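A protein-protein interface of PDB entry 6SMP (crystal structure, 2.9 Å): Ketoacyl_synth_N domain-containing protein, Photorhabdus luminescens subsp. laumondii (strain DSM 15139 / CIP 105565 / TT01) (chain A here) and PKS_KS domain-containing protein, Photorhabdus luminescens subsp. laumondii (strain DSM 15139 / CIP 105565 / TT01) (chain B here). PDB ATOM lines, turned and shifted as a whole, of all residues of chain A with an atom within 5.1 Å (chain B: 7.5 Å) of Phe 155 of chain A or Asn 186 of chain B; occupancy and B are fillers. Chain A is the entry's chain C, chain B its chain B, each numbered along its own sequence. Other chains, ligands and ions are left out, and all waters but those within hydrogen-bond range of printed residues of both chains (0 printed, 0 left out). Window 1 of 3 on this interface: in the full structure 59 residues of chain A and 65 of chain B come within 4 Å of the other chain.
The side-chain hydroxyl (OG) of Ser 183 of chain B is in hydrogen-bond range of the side-chain hydroxyl (OH) of Tyr 168 of chain A, 2.7 Å away. O of Val 184 of chain B lies within hydrogen-bond range of NE2 of Gln 164 of chain A (3.0 Å). The backbone carbonyl oxygen of Asn 186 of chain B is in hydrogen-bond range of the backbone NH of Ser 156 of chain A (3.0 Å). OG1 of Thr 157 of chain A is in hydrogen-bond range of N of Asn 186 of chain B, at 3.1 Å. N of Ser 188 of chain B lies within hydrogen-bond range of O of Thr 154 of chain A (2.8 Å). The side-chain hydroxyl (OG) of Ser 156 of chain A sits close to the side-chain hydroxyl (OG) of Ser 188 of chain B (3.2 Å). OD2 of Asp 196 of chain B lies within salt-bridge range of NZ of Lys 153 of chain A (2.7 Å).
N of Val 125 of chain B sits at hydrogen-bond distance from O of Ser 183 of chain B, at 3.1 Å. The backbone NH of Ile 127 of chain B sits at hydrogen-bond distance from the backbone carbonyl oxygen of Ser 185 of chain B (3.5 Å). The backbone NH (N) of Ser 168 of chain B sits at hydrogen-bond distance from the side-chain carboxylate (OD2) of Asp 166 of chain B (3.1 Å). The backbone carbonyl oxygen (O) of Val 100 of chain A sits at hydrogen-bond distance from the backbone NH (N) of Phe 155 of chain A (2.9 Å). The backbone carbonyl oxygen (O) of Asn 102 of chain A is in hydrogen-bond range of the side-chain hydroxyl (OG) of Ser 156 of chain A (2.7 Å). The side-chain hydroxyl of Thr 157 of chain A is in hydrogen-bond range of the side-chain amide oxygen of Gln 164 of chain A (2.7 Å).
Thr 154 of chain A touches Ile 187 of chain B (O to CA, 3.4 Å). Thr 154 of chain A touches Thr 189 of chain B (N to OG1, 3.6 Å). Phe 155 of chain A touches Asn 186 of chain B (CA to O, 3.4 Å). Phe 155 of chain A touches Ile 187 of chain B (CE2 to CG1, 3.6 Å). Phe 155 of chain A touches Ile 200 of chain B. Ser 156 of chain A touches Phe 167 of chain B. Ser 168 of chain B touches Thr 157 of chain A. Thr 157 of chain A touches Ser 185 of chain B. NE2 of Gln 164 of chain A touches CB of Ser 185 of chain B (3.8 Å). Tyr 168 of chain A touches Ile 200 of chain B.
Of chain B, only Asn 186 (3.4 Å), Ile 187 (3.6 Å) and Ile 200 (3.9 Å) come within 4 Å of Phe 155 of chain A. Asn 186 of chain B touches three residues of chain A. Printed residues of chain A within 4 Å of Ser 188 of chain B: Thr 154 and Ser 156. Of the printed residues of chain A, Ser 183 of chain B touches Tyr 168. Of the printed residues of chain A, Ser 168 of chain B touches Thr 157. Printed residues of chain A within 4 Å of Ile 187 of chain B: Thr 154 and Phe 155. Printed residues of chain B within 4 Å of Ser 156 of chain A: Phe 167 (3.2 Å), Asn 186 (3.0 Å) and Ser 188 (3.2 Å). Ala 193 of chain B touches none of the printed residues of chain A. The nearest residue of chain B that does not touch Phe 155 of chain A is Ser 185 of chain B (4.4 Å). The nearest residue of chain A that does not touch Asn 186 of chain B is Thr 154 of chain A (4.3 Å). The nearest printed residue of chain B that does not touch Ser 156 of chain A is Ser 168 of chain B (4.1 Å).
Hydrophobic or aromatic side chains of chain A within 4 Å of the printed part of chain B: Phe 155 and Tyr 168. Among the printed residues, Asp or Glu carboxylates within 4 Å of a Lys or Arg side-chain nitrogen of the other chain: Lys 153 of chain A with Asp 196 of chain B (2.7 Å).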
ATOM      1  N   TYR A  99     -25.333  14.019  -5.113  1.00  0.00           N
ATOM      2  CA  TYR A  99     -24.950  15.200  -4.350  1.00  0.00           C
ATOM      3  C   TYR A  99     -24.700  14.820  -2.891  1.00  0.00           C
ATOM      4  O   TYR A  99     -25.505  14.116  -2.286  1.00  0.00           O
ATOM      5  CB  TYR A  99     -25.997  16.309  -4.493  1.00  0.00           C
ATOM      6  CG  TYR A  99     -25.799  17.208  -5.688  1.00  0.00           C
ATOM      7  CD1 TYR A  99     -25.851  16.701  -6.978  1.00  0.00           C
ATOM      8  CD2 TYR A  99     -25.559  18.565  -5.535  1.00  0.00           C
ATOM      9  CE1 TYR A  99     -25.665  17.515  -8.083  1.00  0.00           C
ATOM     10  CE2 TYR A  99     -25.374  19.395  -6.630  1.00  0.00           C
ATOM     11  CZ  TYR A  99     -25.427  18.867  -7.909  1.00  0.00           C
ATOM     12  OH  TYR A  99     -25.246  19.676  -8.994  1.00  0.00           O
ATOM     13  N   VAL A 100     -23.576  15.299  -2.336  1.00  0.00           N
ATOM     14  CA  VAL A 100     -23.108  14.871  -1.025  1.00  0.00           C
ATOM     15  C   VAL A 100     -22.691  16.087  -0.200  1.00  0.00           C
ATOM     16  O   VAL A 100     -22.135  17.046  -0.732  1.00  0.00           O
ATOM     17  CB  VAL A 100     -21.948  13.860  -1.142  1.00  0.00           C
ATOM     18  CG1 VAL A 100     -21.445  13.394   0.217  1.00  0.00           C
ATOM     19  CG2 VAL A 100     -22.306  12.662  -2.011  1.00  0.00           C
ATOM     20  N   GLY A 101     -22.958  16.022   1.110  1.00  0.00           N
ATOM     21  CA  GLY A 101     -22.433  16.973   2.076  1.00  0.00           C
ATOM     22  C   GLY A 101     -21.567  16.276   3.123  1.00  0.00           C
ATOM     23  O   GLY A 101     -21.992  15.288   3.718  1.00  0.00           O
ATOM     24  N   ASN A 102     -20.349  16.796   3.335  1.00  0.00           N
ATOM     25  CA  ASN A 102     -19.412  16.211   4.285  1.00  0.00           C
ATOM     26  C   ASN A 102     -18.331  17.224   4.662  1.00  0.00           C
ATOM     27  O   ASN A 102     -17.689  17.798   3.786  1.00  0.00           O
ATOM     28  CB  ASN A 102     -18.779  14.926   3.746  1.00  0.00           C
ATOM     29  CG  ASN A 102     -17.798  14.306   4.718  1.00  0.00           C
ATOM     30  OD1 ASN A 102     -16.596  14.293   4.467  1.00  0.00           O
ATOM     31  ND2 ASN A 102     -18.297  13.805   5.836  1.00  0.00           N
ATOM     32  N   LYS A 153     -21.837  16.516  -7.392  1.00  0.00           N
ATOM     33  CA  LYS A 153     -21.033  17.460  -6.629  1.00  0.00           C
ATOM     34  C   LYS A 153     -20.933  17.031  -5.166  1.00  0.00           C
ATOM     35  O   LYS A 153     -21.760  16.262  -4.678  1.00  0.00           O
ATOM     36  CB  LYS A 153     -21.617  18.874  -6.732  1.00  0.00           C
ATOM     37  CG  LYS A 153     -20.954  19.796  -7.750  1.00  0.00           C
ATOM     38  CD  LYS A 153     -21.385  19.573  -9.190  1.00  0.00           C
ATOM     39  CE  LYS A 153     -20.497  18.621  -9.968  1.00  0.00           C
ATOM     40  NZ  LYS A 153     -19.127  19.151 -10.152  1.00  0.00           N
ATOM     41  N   THR A 154     -19.904  17.549  -4.482  1.00  0.00           N
ATOM     42  CA  THR A 154     -19.731  17.383  -3.047  1.00  0.00           C
ATOM     43  C   THR A 154     -19.443  18.744  -2.417  1.00  0.00           C
ATOM     44  O   THR A 154     -18.528  19.447  -2.842  1.00  0.00           O
ATOM     45  CB  THR A 154     -18.604  16.395  -2.718  1.00  0.00           C
ATOM     46  OG1 THR A 154     -18.774  15.219  -3.510  1.00  0.00           O
ATOM     47  CG2 THR A 154     -18.559  16.018  -1.253  1.00  0.00           C
ATOM     48  N   PHE A 155     -20.237  19.094  -1.398  1.00  0.00           N
ATOM     49  CA  PHE A 155     -20.065  20.332  -0.655  1.00  0.00           C
ATOM     50  C   PHE A 155     -19.459  20.026   0.711  1.00  0.00           C
ATOM     51  O   PHE A 155     -19.739  18.980   1.296  1.00  0.00           O
ATOM     52  CB  PHE A 155     -21.406  21.053  -0.493  1.00  0.00           C
ATOM     53  CG  PHE A 155     -22.010  21.552  -1.780  1.00  0.00           C
ATOM     54  CD1 PHE A 155     -22.844  20.739  -2.534  1.00  0.00           C
ATOM     55  CD2 PHE A 155     -21.741  22.832  -2.241  1.00  0.00           C
ATOM     56  CE1 PHE A 155     -23.396  21.196  -3.722  1.00  0.00           C
ATOM     57  CE2 PHE A 155     -22.296  23.290  -3.428  1.00  0.00           C
ATOM     58  CZ  PHE A 155     -23.120  22.471  -4.166  1.00  0.00           C
ATOM     59  N   SER A 156     -18.634  20.954   1.208  1.00  0.00           N
ATOM     60  CA  SER A 156     -18.007  20.823   2.513  1.00  0.00           C
ATOM     61  C   SER A 156     -18.052  22.143   3.279  1.00  0.00           C
ATOM     62  O   SER A 156     -17.131  22.460   4.030  1.00  0.00           O
ATOM     63  CB  SER A 156     -16.559  20.383   2.340  1.00  0.00           C
ATOM     64  OG  SER A 156     -16.514  19.076   1.760  1.00  0.00           O
ATOM     65  N   THR A 157     -19.135  22.904   3.083  1.00  0.00           N
ATOM     66  CA  THR A 157     -19.358  24.142   3.813  1.00  0.00           C
ATOM     67  C   THR A 157     -19.722  23.800   5.255  1.00  0.00           C
ATOM     68  O   THR A 157     -20.504  22.881   5.489  1.00  0.00           O
ATOM     69  CB  THR A 157     -20.467  24.981   3.162  1.00  0.00           C
ATOM     70  OG1 THR A 157     -20.317  24.949   1.743  1.00  0.00           O
ATOM     71  CG2 THR A 157     -20.476  26.417   3.635  1.00  0.00           C
ATOM     72  N   ALA A 161     -23.326  21.992   4.541  1.00  0.00           N
ATOM     73  CA  ALA A 161     -22.889  21.217   3.386  1.00  0.00           C
ATOM     74  C   ALA A 161     -24.019  20.364   2.809  1.00  0.00           C
ATOM     75  O   ALA A 161     -24.238  20.367   1.598  1.00  0.00           O
ATOM     76  CB  ALA A 161     -21.691  20.374   3.751  1.00  0.00           C
ATOM     77  N   GLN A 164     -27.018  22.399   1.228  1.00  0.00           N
ATOM     78  CA  GLN A 164     -26.668  22.867  -0.105  1.00  0.00           C
ATOM     79  C   GLN A 164     -26.758  21.713  -1.102  1.00  0.00           C
ATOM     80  O   GLN A 164     -27.156  21.917  -2.248  1.00  0.00           O
ATOM     81  CB  GLN A 164     -25.270  23.493  -0.105  1.00  0.00           C
ATOM     82  CG  GLN A 164     -25.210  24.862   0.563  1.00  0.00           C
ATOM     83  CD  GLN A 164     -23.806  25.392   0.734  1.00  0.00           C
ATOM     84  OE1 GLN A 164     -22.827  24.648   0.712  1.00  0.00           O
ATOM     85  NE2 GLN A 164     -23.696  26.698   0.917  1.00  0.00           N
ATOM     86  N   ALA A 165     -26.391  20.506  -0.651  1.00  0.00           N
ATOM     87  CA  ALA A 165     -26.393  19.309  -1.479  1.00  0.00           C
ATOM     88  C   ALA A 165     -27.798  19.004  -2.001  1.00  0.00           C
ATOM     89  O   ALA A 165     -27.951  18.644  -3.166  1.00  0.00           O
ATOM     90  CB  ALA A 165     -25.819  18.145  -0.709  1.00  0.00           C
ATOM     91  N   TYR A 168     -29.129  22.305  -4.405  1.00  0.00           N
ATOM     92  CA  TYR A 168     -28.526  22.407  -5.726  1.00  0.00           C
ATOM     93  C   TYR A 168     -28.776  21.147  -6.554  1.00  0.00           C
ATOM     94  O   TYR A 168     -28.616  21.174  -7.774  1.00  0.00           O
ATOM     95  CB  TYR A 168     -27.043  22.773  -5.631  1.00  0.00           C
ATOM     96  CG  TYR A 168     -26.797  24.187  -5.170  1.00  0.00           C
ATOM     97  CD1 TYR A 168     -27.239  25.267  -5.918  1.00  0.00           C
ATOM     98  CD2 TYR A 168     -26.138  24.446  -3.977  1.00  0.00           C
ATOM     99  CE1 TYR A 168     -27.030  26.571  -5.496  1.00  0.00           C
ATOM    100  CE2 TYR A 168     -25.920  25.743  -3.542  1.00  0.00           C
ATOM    101  CZ  TYR A 168     -26.368  26.808  -4.304  1.00  0.00           C
ATOM    102  OH  TYR A 168     -26.156  28.089  -3.882  1.00  0.00           O
ATOM    103  N   TYR B  96      -3.596  27.977   2.986  1.00  0.00           N
ATOM    104  CA  TYR B  96      -4.863  27.794   2.295  1.00  0.00           C
ATOM    105  C   TYR B  96      -5.677  29.085   2.350  1.00  0.00           C
ATOM    106  O   TYR B  96      -6.197  29.536   1.331  1.00  0.00           O
ATOM    107  CB  TYR B  96      -5.638  26.607   2.879  1.00  0.00           C
ATOM    108  CG  TYR B  96      -7.111  26.582   2.553  1.00  0.00           C
ATOM    109  CD1 TYR B  96      -7.554  26.488   1.242  1.00  0.00           C
ATOM    110  CD2 TYR B  96      -8.068  26.650   3.555  1.00  0.00           C
ATOM    111  CE1 TYR B  96      -8.905  26.470   0.933  1.00  0.00           C
ATOM    112  CE2 TYR B  96      -9.424  26.628   3.264  1.00  0.00           C
ATOM    113  CZ  TYR B  96      -9.844  26.537   1.948  1.00  0.00           C
ATOM    114  OH  TYR B  96     -11.175  26.516   1.649  1.00  0.00           O
ATOM    115  N   VAL B 125     -20.147  34.111  -3.181  1.00  0.00           N
ATOM    116  CA  VAL B 125     -18.787  33.588  -3.160  1.00  0.00           C
ATOM    117  C   VAL B 125     -18.813  32.078  -3.393  1.00  0.00           C
ATOM    118  O   VAL B 125     -19.739  31.396  -2.956  1.00  0.00           O
ATOM    119  CB  VAL B 125     -18.061  33.935  -1.843  1.00  0.00           C
ATOM    120  CG1 VAL B 125     -16.640  33.389  -1.804  1.00  0.00           C
ATOM    121  CG2 VAL B 125     -18.051  35.431  -1.572  1.00  0.00           C
ATOM    122  N   ALA B 126     -17.775  31.569  -4.073  1.00  0.00           N
ATOM    123  CA  ALA B 126     -17.611  30.144  -4.318  1.00  0.00           C
ATOM    124  C   ALA B 126     -16.129  29.799  -4.473  1.00  0.00           C
ATOM    125  O   ALA B 126     -15.613  29.747  -5.588  1.00  0.00           O
ATOM    126  CB  ALA B 126     -18.412  29.730  -5.531  1.00  0.00           C
ATOM    127  N   ILE B 127     -15.457  29.559  -3.339  1.00  0.00           N
ATOM    128  CA  ILE B 127     -14.059  29.148  -3.326  1.00  0.00           C
ATOM    129  C   ILE B 127     -13.990  27.662  -2.981  1.00  0.00           C
ATOM    130  O   ILE B 127     -14.455  27.244  -1.921  1.00  0.00           O
ATOM    131  CB  ILE B 127     -13.222  30.009  -2.355  1.00  0.00           C
ATOM    132  CG1 ILE B 127     -13.392  31.508  -2.627  1.00  0.00           C
ATOM    133  CG2 ILE B 127     -11.758  29.590  -2.389  1.00  0.00           C
ATOM    134  CD1 ILE B 127     -12.640  32.408  -1.672  1.00  0.00           C
ATOM    135  N   ALA B 128     -13.393  26.878  -3.888  1.00  0.00           N
ATOM    136  CA  ALA B 128     -13.312  25.430  -3.757  1.00  0.00           C
ATOM    137  C   ALA B 128     -11.930  25.014  -3.254  1.00  0.00           C
ATOM    138  O   ALA B 128     -10.998  25.818  -3.264  1.00  0.00           O
ATOM    139  CB  ALA B 128     -13.627  24.792  -5.086  1.00  0.00           C
ATOM    140  N   THR B 129     -11.817  23.753  -2.811  1.00  0.00           N
ATOM    141  CA  THR B 129     -10.551  23.168  -2.387  1.00  0.00           C
ATOM    142  C   THR B 129     -10.666  21.646  -2.329  1.00  0.00           C
ATOM    143  O   THR B 129     -11.724  21.112  -1.999  1.00  0.00           O
ATOM    144  CB  THR B 129     -10.075  23.744  -1.045  1.00  0.00           C
ATOM    145  OG1 THR B 129      -8.761  23.250  -0.783  1.00  0.00           O
ATOM    146  CG2 THR B 129     -10.995  23.419   0.112  1.00  0.00           C
ATOM    147  N   ALA B 130      -9.539  20.962  -2.523  1.00  0.00           N
ATOM    148  CA  ALA B 130      -9.484  19.485  -2.464  1.00  0.00           C
ATOM    149  C   ALA B 130      -9.204  18.998  -1.044  1.00  0.00           C
ATOM    150  O   ALA B 130      -9.868  18.058  -0.639  1.00  0.00           O
ATOM    151  CB  ALA B 130      -8.418  18.980  -3.385  1.00  0.00           C
ATOM    152  N   ALA B 132      -8.203  21.489   1.684  1.00  0.00           N
ATOM    153  CA  ALA B 132      -8.317  22.629   2.625  1.00  0.00           C
ATOM    154  C   ALA B 132      -7.065  22.776   3.473  1.00  0.00           C
ATOM    155  O   ALA B 132      -5.982  22.725   2.918  1.00  0.00           O
ATOM    156  CB  ALA B 132      -9.535  22.538   3.486  1.00  0.00           C
ATOM    157  N   ASP B 166     -12.153  23.510   9.462  1.00  0.00           N
ATOM    158  CA  ASP B 166     -13.132  24.206   8.641  1.00  0.00           C
ATOM    159  C   ASP B 166     -12.673  24.170   7.184  1.00  0.00           C
ATOM    160  O   ASP B 166     -11.623  24.718   6.851  1.00  0.00           O
ATOM    161  CB  ASP B 166     -13.352  25.640   9.134  1.00  0.00           C
ATOM    162  CG  ASP B 166     -14.406  26.423   8.364  1.00  0.00           C
ATOM    163  OD1 ASP B 166     -14.460  27.656   8.542  1.00  0.00           O
ATOM    164  OD2 ASP B 166     -15.169  25.799   7.599  1.00  0.00           O
ATOM    165  N   PHE B 167     -13.474  23.524   6.325  1.00  0.00           N
ATOM    166  CA  PHE B 167     -13.164  23.389   4.909  1.00  0.00           C
ATOM    167  C   PHE B 167     -13.411  24.698   4.160  1.00  0.00           C
ATOM    168  O   PHE B 167     -12.740  24.974   3.168  1.00  0.00           O
ATOM    169  CB  PHE B 167     -13.942  22.231   4.278  1.00  0.00           C
ATOM    170  CG  PHE B 167     -13.099  21.055   3.857  1.00  0.00           C
ATOM    171  CD1 PHE B 167     -12.803  20.833   2.520  1.00  0.00           C
ATOM    172  CD2 PHE B 167     -12.593  20.170   4.799  1.00  0.00           C
ATOM    173  CE1 PHE B 167     -12.023  19.752   2.134  1.00  0.00           C
ATOM    174  CE2 PHE B 167     -11.814  19.089   4.413  1.00  0.00           C
ATOM    175  CZ  PHE B 167     -11.530  18.883   3.081  1.00  0.00           C
ATOM    176  N   SER B 168     -14.376  25.493   4.640  1.00  0.00           N
ATOM    177  CA  SER B 168     -14.786  26.715   3.963  1.00  0.00           C
ATOM    178  C   SER B 168     -14.282  27.982   4.654  1.00  0.00           C
ATOM    179  O   SER B 168     -15.016  28.963   4.768  1.00  0.00           O
ATOM    180  CB  SER B 168     -16.311  26.726   3.848  1.00  0.00           C
ATOM    181  OG  SER B 168     -16.913  26.683   5.149  1.00  0.00           O
ATOM    182  N   SER B 169     -13.018  27.953   5.096  1.00  0.00           N
ATOM    183  CA  SER B 169     -12.384  29.090   5.746  1.00  0.00           C
ATOM    184  C   SER B 169     -12.171  30.226   4.747  1.00  0.00           C
ATOM    185  O   SER B 169     -12.426  31.386   5.062  1.00  0.00           O
ATOM    186  CB  SER B 169     -11.034  28.683   6.331  1.00  0.00           C
ATOM    187  OG  SER B 169     -11.199  27.553   7.193  1.00  0.00           O
ATOM    188  N   ALA B 170     -11.716  29.861   3.541  1.00  0.00           N
ATOM    189  CA  ALA B 170     -11.446  30.797   2.462  1.00  0.00           C
ATOM    190  C   ALA B 170     -12.737  31.469   1.996  1.00  0.00           C
ATOM    191  O   ALA B 170     -12.757  32.676   1.769  1.00  0.00           O
ATOM    192  CB  ALA B 170     -10.764  30.073   1.328  1.00  0.00           C
ATOM    193  N   ALA B 171     -13.808  30.675   1.867  1.00  0.00           N
ATOM    194  CA  ALA B 171     -15.081  31.141   1.338  1.00  0.00           C
ATOM    195  C   ALA B 171     -15.719  32.169   2.274  1.00  0.00           C
ATOM    196  O   ALA B 171     -16.170  33.217   1.817  1.00  0.00           O
ATOM    197  CB  ALA B 171     -15.999  29.968   1.094  1.00  0.00           C
ATOM    198  N   THR B 172     -15.740  31.860   3.577  1.00  0.00           N
ATOM    199  CA  THR B 172     -16.444  32.661   4.567  1.00  0.00           C
ATOM    200  C   THR B 172     -15.675  33.945   4.874  1.00  0.00           C
ATOM    201  O   THR B 172     -16.286  34.994   5.069  1.00  0.00           O
ATOM    202  CB  THR B 172     -16.734  31.858   5.842  1.00  0.00           C
ATOM    203  OG1 THR B 172     -15.510  31.319   6.340  1.00  0.00           O
ATOM    204  CG2 THR B 172     -17.731  30.743   5.616  1.00  0.00           C
ATOM    205  N   SER B 183     -25.449  33.445  -1.666  1.00  0.00           N
ATOM    206  CA  SER B 183     -24.850  32.121  -1.551  1.00  0.00           C
ATOM    207  C   SER B 183     -23.327  32.080  -1.412  1.00  0.00           C
ATOM    208  O   SER B 183     -22.603  32.482  -2.323  1.00  0.00           O
ATOM    209  CB  SER B 183     -25.259  31.294  -2.773  1.00  0.00           C
ATOM    210  OG  SER B 183     -24.649  29.997  -2.731  1.00  0.00           O
ATOM    211  N   VAL B 184     -22.863  31.595  -0.253  1.00  0.00           N
ATOM    212  CA  VAL B 184     -21.457  31.315   0.000  1.00  0.00           C
ATOM    213  C   VAL B 184     -21.301  29.800   0.121  1.00  0.00           C
ATOM    214  O   VAL B 184     -22.006  29.166   0.905  1.00  0.00           O
ATOM    215  CB  VAL B 184     -20.948  32.040   1.262  1.00  0.00           C
ATOM    216  CG1 VAL B 184     -19.502  31.687   1.584  1.00  0.00           C
ATOM    217  CG2 VAL B 184     -21.107  33.548   1.146  1.00  0.00           C
ATOM    218  N   SER B 185     -20.381  29.230  -0.667  1.00  0.00           N
ATOM    219  CA  SER B 185     -20.227  27.784  -0.729  1.00  0.00           C
ATOM    220  C   SER B 185     -18.787  27.322  -0.948  1.00  0.00           C
ATOM    221  O   SER B 185     -17.949  28.080  -1.436  1.00  0.00           O
ATOM    222  CB  SER B 185     -21.113  27.230  -1.846  1.00  0.00           C
ATOM    223  OG  SER B 185     -20.714  27.765  -3.114  1.00  0.00           O
ATOM    224  N   ASN B 186     -18.530  26.060  -0.577  1.00  0.00           N
ATOM    225  CA  ASN B 186     -17.257  25.394  -0.802  1.00  0.00           C
ATOM    226  C   ASN B 186     -17.517  24.013  -1.399  1.00  0.00           C
ATOM    227  O   ASN B 186     -18.073  23.140  -0.733  1.00  0.00           O
ATOM    228  CB  ASN B 186     -16.432  25.285   0.484  1.00  0.00           C
ATOM    229  CG  ASN B 186     -15.184  24.442   0.321  1.00  0.00           C
ATOM    230  OD1 ASN B 186     -14.275  24.804  -0.423  1.00  0.00           O
ATOM    231  ND2 ASN B 186     -15.128  23.319   1.017  1.00  0.00           N
ATOM    232  N   ILE B 187     -17.111  23.834  -2.661  1.00  0.00           N
ATOM    233  CA  ILE B 187     -17.217  22.558  -3.353  1.00  0.00           C
ATOM    234  C   ILE B 187     -15.893  21.812  -3.193  1.00  0.00           C
ATOM    235  O   ILE B 187     -14.828  22.382  -3.416  1.00  0.00           O
ATOM    236  CB  ILE B 187     -17.607  22.774  -4.832  1.00  0.00           C
ATOM    237  CG1 ILE B 187     -19.053  23.263  -4.962  1.00  0.00           C
ATOM    238  CG2 ILE B 187     -17.365  21.519  -5.657  1.00  0.00           C
ATOM    239  CD1 ILE B 187     -19.379  23.895  -6.295  1.00  0.00           C
ATOM    240  N   SER B 188     -15.979  20.551  -2.790  1.00  0.00           N
ATOM    241  CA  SER B 188     -14.804  19.758  -2.524  1.00  0.00           C
ATOM    242  C   SER B 188     -14.748  18.559  -3.393  1.00  0.00           C
ATOM    243  O   SER B 188     -14.603  17.507  -2.933  1.00  0.00           O
ATOM    244  CB  SER B 188     -15.028  19.315  -1.098  1.00  0.00           C
ATOM    245  OG  SER B 188     -14.228  20.124  -0.284  1.00  0.00           O
ATOM    246  N   THR B 189     -14.686  18.768  -4.697  1.00  0.00           N
ATOM    247  CA  THR B 189     -14.689  17.668  -5.685  1.00  0.00           C
ATOM    248  C   THR B 189     -13.264  17.319  -6.109  1.00  0.00           C
ATOM    249  O   THR B 189     -13.090  16.795  -7.195  1.00  0.00           O
ATOM    250  CB  THR B 189     -15.602  18.004  -6.859  1.00  0.00           C
ATOM    251  OG1 THR B 189     -16.887  18.242  -6.308  1.00  0.00           O
ATOM    252  CG2 THR B 189     -15.715  16.866  -7.836  1.00  0.00           C
ATOM    253  N   ALA B 193     -12.713  20.579  -8.606  1.00  0.00           N
ATOM    254  CA  ALA B 193     -13.415  21.515  -7.704  1.00  0.00           C
ATOM    255  C   ALA B 193     -13.291  22.959  -8.179  1.00  0.00           C
ATOM    256  O   ALA B 193     -14.174  23.741  -7.873  1.00  0.00           O
ATOM    257  CB  ALA B 193     -12.906  21.341  -6.310  1.00  0.00           C
ATOM    258  N   ASP B 196     -15.796  23.518 -10.933  1.00  0.00           N
ATOM    259  CA  ASP B 196     -17.129  23.302 -10.389  1.00  0.00           C
ATOM    260  C   ASP B 196     -17.584  24.527  -9.598  1.00  0.00           C
ATOM    261  O   ASP B 196     -18.779  24.809  -9.524  1.00  0.00           O
ATOM    262  CB  ASP B 196     -17.190  22.022  -9.550  1.00  0.00           C
ATOM    263  CG  ASP B 196     -16.760  20.777 -10.308  1.00  0.00           C
ATOM    264  OD1 ASP B 196     -16.693  20.838 -11.553  1.00  0.00           O
ATOM    265  OD2 ASP B 196     -16.499  19.754  -9.647  1.00  0.00           O
ATOM    266  N   ALA B 197     -16.614  25.237  -9.009  1.00  0.00           N
ATOM    267  CA  ALA B 197     -16.856  26.502  -8.334  1.00  0.00           C
ATOM    268  C   ALA B 197     -17.228  27.570  -9.362  1.00  0.00           C
ATOM    269  O   ALA B 197     -18.129  28.370  -9.122  1.00  0.00           O
ATOM    270  CB  ALA B 197     -15.640  26.903  -7.537  1.00  0.00           C
ATOM    271  N   ILE B 200     -20.916  26.598 -10.757  1.00  0.00           N
ATOM    272  CA  ILE B 200     -22.049  26.958  -9.917  1.00  0.00           C
ATOM    273  C   ILE B 200     -22.189  28.480  -9.870  1.00  0.00           C
ATOM    274  O   ILE B 200     -23.300  28.997  -9.777  1.00  0.00           O
ATOM    275  CB  ILE B 200     -21.958  26.325  -8.509  1.00  0.00           C
ATOM    276  CG1 ILE B 200     -23.299  26.398  -7.769  1.00  0.00           C
ATOM    277  CG2 ILE B 200     -20.824  26.936  -7.696  1.00  0.00           C
ATOM    278  CD1 ILE B 200     -23.408  25.468  -6.580  1.00  0.00           C
ATOM    279  N   GLY B 216     -13.472  30.695  -7.584  1.00  0.00           N
ATOM    280  CA  GLY B 216     -12.117  30.189  -7.747  1.00  0.00           C
ATOM    281  C   GLY B 216     -11.824  28.995  -6.840  1.00  0.00           C
ATOM    282  O   GLY B 216     -12.743  28.288  -6.426  1.00  0.00           O
ATOM    283  N   ALA B 217     -10.533  28.784  -6.544  1.00  0.00           N
ATOM    284  CA  ALA B 217     -10.086  27.692  -5.691  1.00  0.00           C
ATOM    285  C   ALA B 217      -8.701  27.984  -5.113  1.00  0.00           C
ATOM    286  O   ALA B 217      -7.844  28.539  -5.799  1.00  0.00           O
ATOM    287  CB  ALA B 217     -10.094  26.394  -6.461  1.00  0.00           C
ATOM    288  N   SER B 218      -8.496  27.582  -3.850  1.00  0.00           N
ATOM    289  CA  SER B 218      -7.241  27.771  -3.136  1.00  0.00           C
ATOM    290  C   SER B 218      -6.729  26.438  -2.589  1.00  0.00           C
ATOM    291  O   SER B 218      -7.518  25.611  -2.136  1.00  0.00           O
ATOM    292  CB  SER B 218      -7.475  28.721  -1.965  1.00  0.00           C
ATOM    293  OG  SER B 218      -6.218  29.141  -1.421  1.00  0.00           O
